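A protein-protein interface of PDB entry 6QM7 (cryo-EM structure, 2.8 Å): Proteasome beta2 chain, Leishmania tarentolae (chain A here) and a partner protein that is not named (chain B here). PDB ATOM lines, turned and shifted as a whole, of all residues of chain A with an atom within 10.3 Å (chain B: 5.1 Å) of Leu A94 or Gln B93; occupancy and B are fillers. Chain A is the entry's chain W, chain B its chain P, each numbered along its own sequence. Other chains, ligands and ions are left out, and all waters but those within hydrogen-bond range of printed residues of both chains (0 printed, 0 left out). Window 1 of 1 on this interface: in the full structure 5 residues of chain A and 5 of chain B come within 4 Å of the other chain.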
ATOM      1  N   TYR A  65      -9.163 -14.425  18.162  1.00  0.00           N
ATOM      2  CA  TYR A  65      -8.737 -14.153  19.555  1.00  0.00           C
ATOM      3  C   TYR A  65      -7.988 -12.825  19.566  1.00  0.00           C
ATOM      4  O   TYR A  65      -7.060 -12.665  18.743  1.00  0.00           O
ATOM      5  CB  TYR A  65      -7.874 -15.298  20.080  1.00  0.00           C
ATOM      6  CG  TYR A  65      -7.137 -15.011  21.359  1.00  0.00           C
ATOM      7  CD1 TYR A  65      -7.580 -15.522  22.571  1.00  0.00           C
ATOM      8  CD2 TYR A  65      -5.968 -14.262  21.351  1.00  0.00           C
ATOM      9  CE1 TYR A  65      -6.886 -15.283  23.751  1.00  0.00           C
ATOM     10  CE2 TYR A  65      -5.265 -14.012  22.520  1.00  0.00           C
ATOM     11  CZ  TYR A  65      -5.729 -14.520  23.723  1.00  0.00           C
ATOM     12  OH  TYR A  65      -5.025 -14.279  24.862  1.00  0.00           O
ATOM     13  N   MET A  66      -8.408 -11.905  20.436  1.00  0.00           N
ATOM     14  CA  MET A  66      -7.696 -10.637  20.727  1.00  0.00           C
ATOM     15  C   MET A  66      -7.050 -10.757  22.111  1.00  0.00           C
ATOM     16  O   MET A  66      -5.844 -10.472  22.258  1.00  0.00           O
ATOM     17  CB  MET A  66      -8.662  -9.449  20.684  1.00  0.00           C
ATOM     18  CG  MET A  66      -7.966  -8.097  20.596  1.00  0.00           C
ATOM     19  SD  MET A  66      -8.011  -7.323  18.960  1.00  0.00           S
ATOM     20  CE  MET A  66      -7.793  -8.753  17.906  1.00  0.00           C
ATOM     21  N   ALA A  67      -7.832 -11.188  23.098  1.00  0.00           N
ATOM     22  CA  ALA A  67      -7.378 -11.419  24.485  1.00  0.00           C
ATOM     23  C   ALA A  67      -8.267 -12.473  25.131  1.00  0.00           C
ATOM     24  O   ALA A  67      -9.263 -12.873  24.542  1.00  0.00           O
ATOM     25  CB  ALA A  67      -7.417 -10.112  25.223  1.00  0.00           C
ATOM     26  N   PRO A  68      -7.946 -12.974  26.341  1.00  0.00           N
ATOM     27  CA  PRO A  68      -8.810 -13.935  27.033  1.00  0.00           C
ATOM     28  C   PRO A  68     -10.288 -13.529  27.108  1.00  0.00           C
ATOM     29  O   PRO A  68     -11.135 -14.404  27.002  1.00  0.00           O
ATOM     30  CB  PRO A  68      -8.228 -13.932  28.452  1.00  0.00           C
ATOM     31  CG  PRO A  68      -6.759 -13.691  28.212  1.00  0.00           C
ATOM     32  CD  PRO A  68      -6.739 -12.652  27.113  1.00  0.00           C
ATOM     33  N   THR A  85      -5.365  -7.420  13.586  1.00  0.00           N
ATOM     34  CA  THR A  85      -5.931  -8.177  14.725  1.00  0.00           C
ATOM     35  C   THR A  85      -4.795  -8.903  15.460  1.00  0.00           C
ATOM     36  O   THR A  85      -4.810  -8.887  16.697  1.00  0.00           O
ATOM     37  CB  THR A  85      -7.096  -9.039  14.226  1.00  0.00           C
ATOM     38  OG1 THR A  85      -8.312  -8.373  14.567  1.00  0.00           O
ATOM     39  CG2 THR A  85      -7.111 -10.438  14.789  1.00  0.00           C
ATOM     40  N   ASN A  86      -3.860  -9.526  14.733  1.00  0.00           N
ATOM     41  CA  ASN A  86      -2.677 -10.205  15.329  1.00  0.00           C
ATOM     42  C   ASN A  86      -1.829  -9.162  16.050  1.00  0.00           C
ATOM     43  O   ASN A  86      -1.497  -9.396  17.217  1.00  0.00           O
ATOM     44  CB  ASN A  86      -1.846 -10.987  14.306  1.00  0.00           C
ATOM     45  CG  ASN A  86      -2.416 -12.361  14.017  1.00  0.00           C
ATOM     46  OD1 ASN A  86      -2.835 -13.076  14.924  1.00  0.00           O
ATOM     47  ND2 ASN A  86      -2.446 -12.750  12.754  1.00  0.00           N
ATOM     48  N   MET A  87      -1.512  -8.064  15.365  1.00  0.00           N
ATOM     49  CA  MET A  87      -0.613  -6.988  15.862  1.00  0.00           C
ATOM     50  C   MET A  87      -1.111  -6.507  17.221  1.00  0.00           C
ATOM     51  O   MET A  87      -0.278  -6.326  18.131  1.00  0.00           O
ATOM     52  CB  MET A  87      -0.574  -5.792  14.909  1.00  0.00           C
ATOM     53  CG  MET A  87      -0.195  -4.469  15.578  1.00  0.00           C
ATOM     54  SD  MET A  87      -0.706  -3.051  14.585  1.00  0.00           S
ATOM     55  CE  MET A  87       0.328  -3.327  13.143  1.00  0.00           C
ATOM     56  N   VAL A  88      -2.405  -6.235  17.308  1.00  0.00           N
ATOM     57  CA  VAL A  88      -3.038  -5.660  18.520  1.00  0.00           C
ATOM     58  C   VAL A  88      -3.045  -6.744  19.597  1.00  0.00           C
ATOM     59  O   VAL A  88      -2.523  -6.465  20.682  1.00  0.00           O
ATOM     60  CB  VAL A  88      -4.435  -5.098  18.206  1.00  0.00           C
ATOM     61  CG1 VAL A  88      -5.313  -4.969  19.442  1.00  0.00           C
ATOM     62  CG2 VAL A  88      -4.305  -3.758  17.496  1.00  0.00           C
ATOM     63  N   SER A  89      -3.574  -7.933  19.304  1.00  0.00           N
ATOM     64  CA  SER A  89      -3.673  -9.043  20.288  1.00  0.00           C
ATOM     65  C   SER A  89      -2.318  -9.227  20.969  1.00  0.00           C
ATOM     66  O   SER A  89      -2.299  -9.465  22.194  1.00  0.00           O
ATOM     67  CB  SER A  89      -4.159 -10.337  19.683  1.00  0.00           C
ATOM     68  OG  SER A  89      -3.093 -11.071  19.108  1.00  0.00           O
ATOM     69  N   SER A  90      -1.242  -9.116  20.192  1.00  0.00           N
ATOM     70  CA  SER A  90       0.159  -9.209  20.660  1.00  0.00           C
ATOM     71  C   SER A  90       0.462  -8.038  21.595  1.00  0.00           C
ATOM     72  O   SER A  90       0.946  -8.294  22.706  1.00  0.00           O
ATOM     73  CB  SER A  90       1.116  -9.245  19.514  1.00  0.00           C
ATOM     74  OG  SER A  90       2.455  -9.235  19.980  1.00  0.00           O
ATOM     75  N   HIS A  91       0.183  -6.811  21.171  1.00  0.00           N
ATOM     76  CA  HIS A  91       0.394  -5.595  21.994  1.00  0.00           C
ATOM     77  C   HIS A  91      -0.424  -5.697  23.286  1.00  0.00           C
ATOM     78  O   HIS A  91       0.129  -5.437  24.343  1.00  0.00           O
ATOM     79  CB  HIS A  91       0.076  -4.330  21.197  1.00  0.00           C
ATOM     80  CG  HIS A  91       0.555  -3.077  21.845  1.00  0.00           C
ATOM     81  ND1 HIS A  91       0.443  -1.855  21.220  1.00  0.00           N
ATOM     82  CD2 HIS A  91       1.147  -2.846  23.041  1.00  0.00           C
ATOM     83  CE1 HIS A  91       0.929  -0.916  22.012  1.00  0.00           C
ATOM     84  NE2 HIS A  91       1.371  -1.505  23.140  1.00  0.00           N
ATOM     85  N   LEU A  92      -1.687  -6.088  23.218  1.00  0.00           N
ATOM     86  CA  LEU A  92      -2.524  -6.291  24.424  1.00  0.00           C
ATOM     87  C   LEU A  92      -1.861  -7.300  25.357  1.00  0.00           C
ATOM     88  O   LEU A  92      -1.972  -7.096  26.574  1.00  0.00           O
ATOM     89  CB  LEU A  92      -3.918  -6.794  24.035  1.00  0.00           C
ATOM     90  CG  LEU A  92      -4.806  -5.772  23.342  1.00  0.00           C
ATOM     91  CD1 LEU A  92      -6.174  -6.355  23.057  1.00  0.00           C
ATOM     92  CD2 LEU A  92      -4.913  -4.496  24.171  1.00  0.00           C
ATOM     93  N   ALA A  93      -1.283  -8.372  24.813  1.00  0.00           N
ATOM     94  CA  ALA A  93      -0.699  -9.490  25.591  1.00  0.00           C
ATOM     95  C   ALA A  93       0.534  -8.996  26.342  1.00  0.00           C
ATOM     96  O   ALA A  93       0.740  -9.405  27.485  1.00  0.00           O
ATOM     97  CB  ALA A  93      -0.355 -10.639  24.674  1.00  0.00           C
ATOM     98  N   LEU A  94       1.333  -8.186  25.657  1.00  0.00           N
ATOM     99  CA  LEU A  94       2.597  -7.585  26.145  1.00  0.00           C
ATOM    100  C   LEU A  94       2.271  -6.594  27.247  1.00  0.00           C
ATOM    101  O   LEU A  94       3.031  -6.516  28.209  1.00  0.00           O
ATOM    102  CB  LEU A  94       3.266  -6.852  24.982  1.00  0.00           C
ATOM    103  CG  LEU A  94       4.730  -7.194  24.751  1.00  0.00           C
ATOM    104  CD1 LEU A  94       5.214  -6.478  23.499  1.00  0.00           C
ATOM    105  CD2 LEU A  94       5.569  -6.812  25.965  1.00  0.00           C
ATOM    106  N   HIS A  95       1.188  -5.850  27.047  1.00  0.00           N
ATOM    107  CA  HIS A  95       0.655  -4.797  27.937  1.00  0.00           C
ATOM    108  C   HIS A  95       0.025  -5.434  29.158  1.00  0.00           C
ATOM    109  O   HIS A  95      -0.064  -4.761  30.172  1.00  0.00           O
ATOM    110  CB  HIS A  95      -0.373  -3.951  27.191  1.00  0.00           C
ATOM    111  CG  HIS A  95      -0.802  -2.740  27.940  1.00  0.00           C
ATOM    112  ND1 HIS A  95      -2.136  -2.469  28.174  1.00  0.00           N
ATOM    113  CD2 HIS A  95      -0.084  -1.754  28.528  1.00  0.00           C
ATOM    114  CE1 HIS A  95      -2.232  -1.358  28.869  1.00  0.00           C
ATOM    115  NE2 HIS A  95      -0.978  -0.898  29.106  1.00  0.00           N
ATOM    116  N   ARG A  96      -0.422  -6.676  29.036  1.00  0.00           N
ATOM    117  CA  ARG A  96      -1.100  -7.433  30.120  1.00  0.00           C
ATOM    118  C   ARG A  96      -0.046  -7.927  31.110  1.00  0.00           C
ATOM    119  O   ARG A  96      -0.396  -8.187  32.273  1.00  0.00           O
ATOM    120  CB  ARG A  96      -1.895  -8.579  29.498  1.00  0.00           C
ATOM    121  CG  ARG A  96      -3.026  -9.111  30.353  1.00  0.00           C
ATOM    122  CD  ARG A  96      -4.131  -9.741  29.529  1.00  0.00           C
ATOM    123  NE  ARG A  96      -3.641 -10.789  28.646  1.00  0.00           N
ATOM    124  CZ  ARG A  96      -3.657 -10.758  27.321  1.00  0.00           C
ATOM    125  NH1 ARG A  96      -4.145  -9.714  26.667  1.00  0.00           N
ATOM    126  NH2 ARG A  96      -3.181 -11.792  26.646  1.00  0.00           N
ATOM    127  N   LEU A  97       1.195  -8.067  30.656  1.00  0.00           N
ATOM    128  CA  LEU A  97       2.336  -8.478  31.504  1.00  0.00           C
ATOM    129  C   LEU A  97       2.866  -7.254  32.245  1.00  0.00           C
ATOM    130  O   LEU A  97       3.364  -7.417  33.383  1.00  0.00           O
ATOM    131  CB  LEU A  97       3.409  -9.109  30.619  1.00  0.00           C
ATOM    132  CG  LEU A  97       2.969 -10.385  29.919  1.00  0.00           C
ATOM    133  CD1 LEU A  97       4.037 -10.859  28.950  1.00  0.00           C
ATOM    134  CD2 LEU A  97       2.626 -11.469  30.929  1.00  0.00           C
ATOM    135  N   GLU A  98       2.770  -6.086  31.617  1.00  0.00           N
ATOM    136  CA  GLU A  98       3.211  -4.803  32.208  1.00  0.00           C
ATOM    137  C   GLU A  98       2.231  -4.396  33.315  1.00  0.00           C
ATOM    138  O   GLU A  98       2.690  -4.052  34.408  1.00  0.00           O
ATOM    139  CB  GLU A  98       3.324  -3.751  31.106  1.00  0.00           C
ATOM    140  CG  GLU A  98       3.903  -2.431  31.584  1.00  0.00           C
ATOM    141  CD  GLU A  98       4.213  -1.447  30.468  1.00  0.00           C
ATOM    142  OE1 GLU A  98       3.384  -1.342  29.521  1.00  0.00           O
ATOM    143  OE2 GLU A  98       5.276  -0.784  30.543  1.00  0.00           O
ATOM    144  N   THR A  99       0.930  -4.457  33.043  1.00  0.00           N
ATOM    145  CA  THR A  99      -0.148  -4.005  33.957  1.00  0.00           C
ATOM    146  C   THR A  99      -0.432  -5.081  35.010  1.00  0.00           C
ATOM    147  O   THR A  99      -0.739  -4.707  36.146  1.00  0.00           O
ATOM    148  CB  THR A  99      -1.421  -3.651  33.172  1.00  0.00           C
ATOM    149  OG1 THR A  99      -1.856  -4.809  32.457  1.00  0.00           O
ATOM    150  CG2 THR A  99      -1.243  -2.520  32.181  1.00  0.00           C
ATOM    151  N   GLY A 100      -0.356  -6.359  34.638  1.00  0.00           N
ATOM    152  CA  GLY A 100      -0.808  -7.495  35.468  1.00  0.00           C
ATOM    153  C   GLY A 100      -2.323  -7.527  35.601  1.00  0.00           C
ATOM    154  O   GLY A 100      -2.827  -7.997  36.639  1.00  0.00           O
ATOM    155  N   LYS A 101      -3.019  -7.081  34.560  1.00  0.00           N
ATOM    156  CA  LYS A 101      -4.420  -6.594  34.608  1.00  0.00           C
ATOM    157  C   LYS A 101      -5.117  -7.047  33.327  1.00  0.00           C
ATOM    158  O   LYS A 101      -4.524  -6.845  32.254  1.00  0.00           O
ATOM    159  CB  LYS A 101      -4.411  -5.063  34.683  1.00  0.00           C
ATOM    160  CG  LYS A 101      -5.236  -4.439  35.792  1.00  0.00           C
ATOM    161  CD  LYS A 101      -4.537  -4.424  37.126  1.00  0.00           C
ATOM    162  CE  LYS A 101      -5.331  -3.690  38.184  1.00  0.00           C
ATOM    163  NZ  LYS A 101      -4.657  -3.741  39.504  1.00  0.00           N
ATOM    164  N   GLN A 102      -6.326  -7.603  33.420  1.00  0.00           N
ATOM    165  CA  GLN A 102      -7.046  -8.120  32.229  1.00  0.00           C
ATOM    166  C   GLN A 102      -7.189  -6.944  31.259  1.00  0.00           C
ATOM    167  O   GLN A 102      -7.390  -5.823  31.739  1.00  0.00           O
ATOM    168  CB  GLN A 102      -8.360  -8.808  32.619  1.00  0.00           C
ATOM    169  CG  GLN A 102      -9.627  -8.094  32.166  1.00  0.00           C
ATOM    170  CD  GLN A 102     -10.862  -8.863  32.560  1.00  0.00           C
ATOM    171  OE1 GLN A 102     -11.787  -8.316  33.168  1.00  0.00           O
ATOM    172  NE2 GLN A 102     -10.877 -10.143  32.217  1.00  0.00           N
ATOM    173  N   SER A 103      -7.009  -7.177  29.961  1.00  0.00           N
ATOM    174  CA  SER A 103      -7.039  -6.103  28.936  1.00  0.00           C
ATOM    175  C   SER A 103      -8.466  -5.565  28.835  1.00  0.00           C
ATOM    176  O   SER A 103      -9.412  -6.358  28.856  1.00  0.00           O
ATOM    177  CB  SER A 103      -6.493  -6.537  27.594  1.00  0.00           C
ATOM    178  OG  SER A 103      -6.689  -7.921  27.380  1.00  0.00           O
ATOM    179  N   GLU A 107      -8.979  -0.347  25.460  1.00  0.00           N
ATOM    180  CA  GLU A 107      -7.542  -0.386  25.076  1.00  0.00           C
ATOM    181  C   GLU A 107      -7.453  -1.032  23.693  1.00  0.00           C
ATOM    182  O   GLU A 107      -6.801  -0.455  22.818  1.00  0.00           O
ATOM    183  CB  GLU A 107      -6.664  -1.187  26.037  1.00  0.00           C
ATOM    184  CG  GLU A 107      -6.568  -0.647  27.456  1.00  0.00           C
ATOM    185  CD  GLU A 107      -5.882  -1.606  28.438  1.00  0.00           C
ATOM    186  OE1 GLU A 107      -5.305  -2.636  27.985  1.00  0.00           O
ATOM    187  OE2 GLU A 107      -5.922  -1.334  29.661  1.00  0.00           O
ATOM    188  N   LEU A 111      -6.279   0.944  20.160  1.00  0.00           N
ATOM    189  CA  LEU A 111      -5.106   0.451  19.392  1.00  0.00           C
ATOM    190  C   LEU A 111      -5.489   0.217  17.938  1.00  0.00           C
ATOM    191  O   LEU A 111      -4.675   0.557  17.081  1.00  0.00           O
ATOM    192  CB  LEU A 111      -4.595  -0.844  20.012  1.00  0.00           C
ATOM    193  CG  LEU A 111      -3.981  -0.678  21.395  1.00  0.00           C
ATOM    194  CD1 LEU A 111      -3.728  -2.046  22.016  1.00  0.00           C
ATOM    195  CD2 LEU A 111      -2.707   0.139  21.339  1.00  0.00           C
ATOM    196  N   ASP B  67       6.229 -15.112  28.450  1.00  0.00           N
ATOM    197  CA  ASP B  67       5.076 -15.477  27.593  1.00  0.00           C
ATOM    198  C   ASP B  67       4.366 -16.666  28.223  1.00  0.00           C
ATOM    199  O   ASP B  67       4.811 -17.109  29.265  1.00  0.00           O
ATOM    200  CB  ASP B  67       5.517 -15.800  26.166  1.00  0.00           C
ATOM    201  CG  ASP B  67       4.489 -15.460  25.087  1.00  0.00           C
ATOM    202  OD1 ASP B  67       3.435 -14.858  25.421  1.00  0.00           O
ATOM    203  OD2 ASP B  67       4.739 -15.814  23.903  1.00  0.00           O
ATOM    204  N   ASP B  86      11.528  -6.854  29.811  1.00  0.00           N
ATOM    205  CA  ASP B  86      10.648  -6.086  28.891  1.00  0.00           C
ATOM    206  C   ASP B  86      11.028  -6.440  27.454  1.00  0.00           C
ATOM    207  O   ASP B  86      10.096  -6.623  26.624  1.00  0.00           O
ATOM    208  CB  ASP B  86      10.689  -4.580  29.169  1.00  0.00           C
ATOM    209  CG  ASP B  86       9.849  -4.124  30.368  1.00  0.00           C
ATOM    210  OD1 ASP B  86       8.881  -4.860  30.766  1.00  0.00           O
ATOM    211  OD2 ASP B  86      10.165  -3.029  30.915  1.00  0.00           O
ATOM    212  N   ARG B  89      10.112 -10.117  26.658  1.00  0.00           N
ATOM    213  CA  ARG B  89       8.645 -10.178  26.439  1.00  0.00           C
ATOM    214  C   ARG B  89       8.335  -9.737  25.007  1.00  0.00           C
ATOM    215  O   ARG B  89       7.520 -10.400  24.355  1.00  0.00           O
ATOM    216  CB  ARG B  89       7.907  -9.329  27.471  1.00  0.00           C
ATOM    217  CG  ARG B  89       7.749 -10.028  28.807  1.00  0.00           C
ATOM    218  CD  ARG B  89       7.456  -9.031  29.895  1.00  0.00           C
ATOM    219  NE  ARG B  89       7.048  -9.713  31.099  1.00  0.00           N
ATOM    220  CZ  ARG B  89       6.712  -9.109  32.225  1.00  0.00           C
ATOM    221  NH1 ARG B  89       6.751  -7.789  32.316  1.00  0.00           N
ATOM    222  NH2 ARG B  89       6.341  -9.832  33.267  1.00  0.00           N
ATOM    223  N   LYS B  90       8.978  -8.658  24.562  1.00  0.00           N
ATOM    224  CA  LYS B  90       8.867  -8.128  23.182  1.00  0.00           C
ATOM    225  C   LYS B  90       9.262  -9.233  22.199  1.00  0.00           C
ATOM    226  O   LYS B  90       8.517  -9.426  21.222  1.00  0.00           O
ATOM    227  CB  LYS B  90       9.737  -6.881  23.006  1.00  0.00           C
ATOM    228  CG  LYS B  90       9.251  -5.899  21.949  1.00  0.00           C
ATOM    229  CD  LYS B  90       9.551  -4.450  22.293  1.00  0.00           C
ATOM    230  CE  LYS B  90       8.679  -3.921  23.424  1.00  0.00           C
ATOM    231  NZ  LYS B  90       9.469  -3.171  24.433  1.00  0.00           N
ATOM    232  N   ASN B  91      10.370  -9.927  22.466  1.00  0.00           N
ATOM    233  CA  ASN B  91      10.942 -10.981  21.589  1.00  0.00           C
ATOM    234  C   ASN B  91       9.982 -12.168  21.482  1.00  0.00           C
ATOM    235  O   ASN B  91       9.844 -12.687  20.366  1.00  0.00           O
ATOM    236  CB  ASN B  91      12.330 -11.428  22.052  1.00  0.00           C
ATOM    237  CG  ASN B  91      13.385 -10.385  21.750  1.00  0.00           C
ATOM    238  OD1 ASN B  91      13.222  -9.585  20.832  1.00  0.00           O
ATOM    239  ND2 ASN B  91      14.467 -10.379  22.512  1.00  0.00           N
ATOM    240  N   CYS B  92       9.350 -12.588  22.574  1.00  0.00           N
ATOM    241  CA  CYS B  92       8.380 -13.712  22.550  1.00  0.00           C
ATOM    242  C   CYS B  92       7.190 -13.352  21.658  1.00  0.00           C
ATOM    243  O   CYS B  92       6.736 -14.222  20.886  1.00  0.00           O
ATOM    244  CB  CYS B  92       7.893 -14.072  23.943  1.00  0.00           C
ATOM    245  SG  CYS B  92       9.258 -14.544  25.030  1.00  0.00           S
ATOM    246  N   GLN B  93       6.729 -12.107  21.755  1.00  0.00           N
ATOM    247  CA  GLN B  93       5.597 -11.584  20.960  1.00  0.00           C
ATOM    248  C   GLN B  93       6.025 -11.401  19.505  1.00  0.00           C
ATOM    249  O   GLN B  93       5.236 -11.808  18.644  1.00  0.00           O
ATOM    250  CB  GLN B  93       5.039 -10.301  21.572  1.00  0.00           C
ATOM    251  CG  GLN B  93       4.120 -10.544  22.767  1.00  0.00           C
ATOM    252  CD  GLN B  93       3.123 -11.661  22.565  1.00  0.00           C
ATOM    253  OE1 GLN B  93       2.387 -11.693  21.583  1.00  0.00           O
ATOM    254  NE2 GLN B  93       3.099 -12.605  23.492  1.00  0.00           N
ATOM    255  N   GLN B  94       7.200 -10.826  19.237  1.00  0.00           N
ATOM    256  CA  GLN B  94       7.705 -10.634  17.849  1.00  0.00           C
ATOM    257  C   GLN B  94       7.802 -11.986  17.149  1.00  0.00           C
ATOM    258  O   GLN B  94       7.427 -12.092  15.973  1.00  0.00           O
ATOM    259  CB  GLN B  94       9.084  -9.992  17.817  1.00  0.00           C
ATOM    260  CG  GLN B  94       9.059  -8.469  17.835  1.00  0.00           C
ATOM    261  CD  GLN B  94      10.477  -7.945  17.913  1.00  0.00           C
ATOM    262  OE1 GLN B  94      11.349  -8.326  17.124  1.00  0.00           O
ATOM    263  NE2 GLN B  94      10.728  -7.088  18.893  1.00  0.00           N
ATOM    264  N   TYR B  95       8.303 -12.978  17.861  1.00  0.00           N
ATOM    265  CA  TYR B  95       8.441 -14.362  17.367  1.00  0.00           C
ATOM    266  C   TYR B  95       7.066 -14.940  17.057  1.00  0.00           C
ATOM    267  O   TYR B  95       6.983 -15.618  16.047  1.00  0.00           O
ATOM    268  CB  TYR B  95       9.190 -15.225  18.382  1.00  0.00           C
ATOM    269  CG  TYR B  95       9.621 -16.547  17.821  1.00  0.00           C
ATOM    270  CD1 TYR B  95      10.898 -16.737  17.325  1.00  0.00           C
ATOM    271  CD2 TYR B  95       8.725 -17.597  17.738  1.00  0.00           C
ATOM    272  CE1 TYR B  95      11.289 -17.958  16.810  1.00  0.00           C
ATOM    273  CE2 TYR B  95       9.095 -18.820  17.207  1.00  0.00           C
ATOM    274  CZ  TYR B  95      10.384 -19.002  16.746  1.00  0.00           C
ATOM    275  OH  TYR B  95      10.695 -20.226  16.238  1.00  0.00           O
ATOM    276  N   LYS B  96       6.066 -14.749  17.920  1.00  0.00           N
ATOM    277  CA  LYS B  96       4.692 -15.276  17.708  1.00  0.00           C
ATOM    278  C   LYS B  96       4.103 -14.621  16.469  1.00  0.00           C
ATOM    279  O   LYS B  96       3.510 -15.325  15.655  1.00  0.00           O
ATOM    280  CB  LYS B  96       3.745 -14.971  18.869  1.00  0.00           C
ATOM    281  CG  LYS B  96       3.817 -15.933  20.041  1.00  0.00           C
ATOM    282  CD  LYS B  96       2.471 -16.429  20.488  1.00  0.00           C
ATOM    283  CE  LYS B  96       2.559 -17.334  21.702  1.00  0.00           C
ATOM    284  NZ  LYS B  96       2.337 -16.584  22.962  1.00  0.00           N
ATOM    285  N   LEU B  97       4.241 -13.307  16.350  1.00  0.00           N
ATOM    286  CA  LEU B  97       3.731 -12.555  15.181  1.00  0.00           C
ATOM    287  C   LEU B  97       4.316 -13.157  13.911  1.00  0.00           C
ATOM    288  O   LEU B  97       3.537 -13.387  12.966  1.00  0.00           O
ATOM    289  CB  LEU B  97       4.098 -11.080  15.311  1.00  0.00           C
ATOM    290  CG  LEU B  97       3.223 -10.328  16.305  1.00  0.00           C
ATOM    291  CD1 LEU B  97       3.772  -8.930  16.568  1.00  0.00           C
ATOM    292  CD2 LEU B  97       1.784 -10.284  15.819  1.00  0.00           C
ATOM    293  N   MET B  98       5.622 -13.406  13.887  1.00  0.00           N
ATOM    294  CA  MET B  98       6.262 -13.957  12.674  1.00  0.00           C
ATOM    295  C   MET B  98       5.764 -15.382  12.448  1.00  0.00           C
ATOM    296  O   MET B  98       5.163 -15.604  11.398  1.00  0.00           O
ATOM    297  CB  MET B  98       7.783 -13.956  12.743  1.00  0.00           C
ATOM    298  CG  MET B  98       8.407 -14.100  11.373  1.00  0.00           C
ATOM    299  SD  MET B  98       9.504 -12.704  11.013  1.00  0.00           S
ATOM    300  CE  MET B  98      10.642 -12.827  12.401  1.00  0.00           C
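The backbone carbonyl oxygen (O) of Asn A86 sits at hydrogen-bond distance from the side-chain hydroxyl (OG) of Ser A89 (3.0 Å). The side-chain carboxylate (OD1) of Asp B86 is in salt-bridge range of the guanidinium group (NH1) of Arg B89, at 3.9 Å. The side-chain amide nitrogen (NE2) of Gln B93 is in hydrogen-bond range of the side-chain carboxylate (OD1) of Asp B67, at 3.0 Å.
Among the printed residues, merely in contact across the chains: Leu A97 with Arg B89 (3.6 Å), Ser A90 with Leu B97 (3.7 Å), Asn A86 with Leu B97 (3.7 Å), Leu A94 with Arg B89 (3.8 Å), Leu A94 with Gln B93 (3.9 Å) and Met A87 with Leu B97 (3.9998 Å).
OG of Ser A90 lies within hydrogen-bond range of OE1 of Gln B93.
Of the 12 printed residues of chain B, 3 touch a printed residue of chain A. Of the 25 printed residues of chain A, 5 touch a printed residue of chain B. Printed residues of chain A that touch a printed residue of chain B: Asn A86, Met A87, Ser A90, Leu A94 and Leu A97. Hydrophobic or aromatic side chains of chain A within 4 Å of the printed part of chain B: Leu A94 and Leu A97.
Leu A94 touches just these residues of chain B: Arg B89 (3.8 Å) and Gln B93 (3.9 Å). Of chain A, only Ser A90 and Leu A94 come within 4 Å of Gln B93. No residue of chain A comes within 4 Å of Cys B92. Lys B96 touches none of the printed residues of chain A. Printed residues of chain B within 4 Å of Met A87: Leu B97. Of the printed residues of chain A, Arg B89 touches Leu A94 and Leu A97. Of the printed residues of chain A, Leu B97 touches Asn A86 (3.7 Å), Met A87 (3.9998 Å) and Ser A90 (3.7 Å). Printed residues of chain B within 4 Å of Asn A86: Leu B97. Of the printed residues of chain B, Ser A90 touches Gln B93 and Leu B97. Met A66 touches none of the printed residues of chain B. Leu A111 touches none of the printed residues of chain B. The nearest residue of chain B that does not touch Leu A94 is Lys B90 (4.02 Å). The nearest printed residue of chain B that does not touch Met A87 is Gln B93 (6.9 Å).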
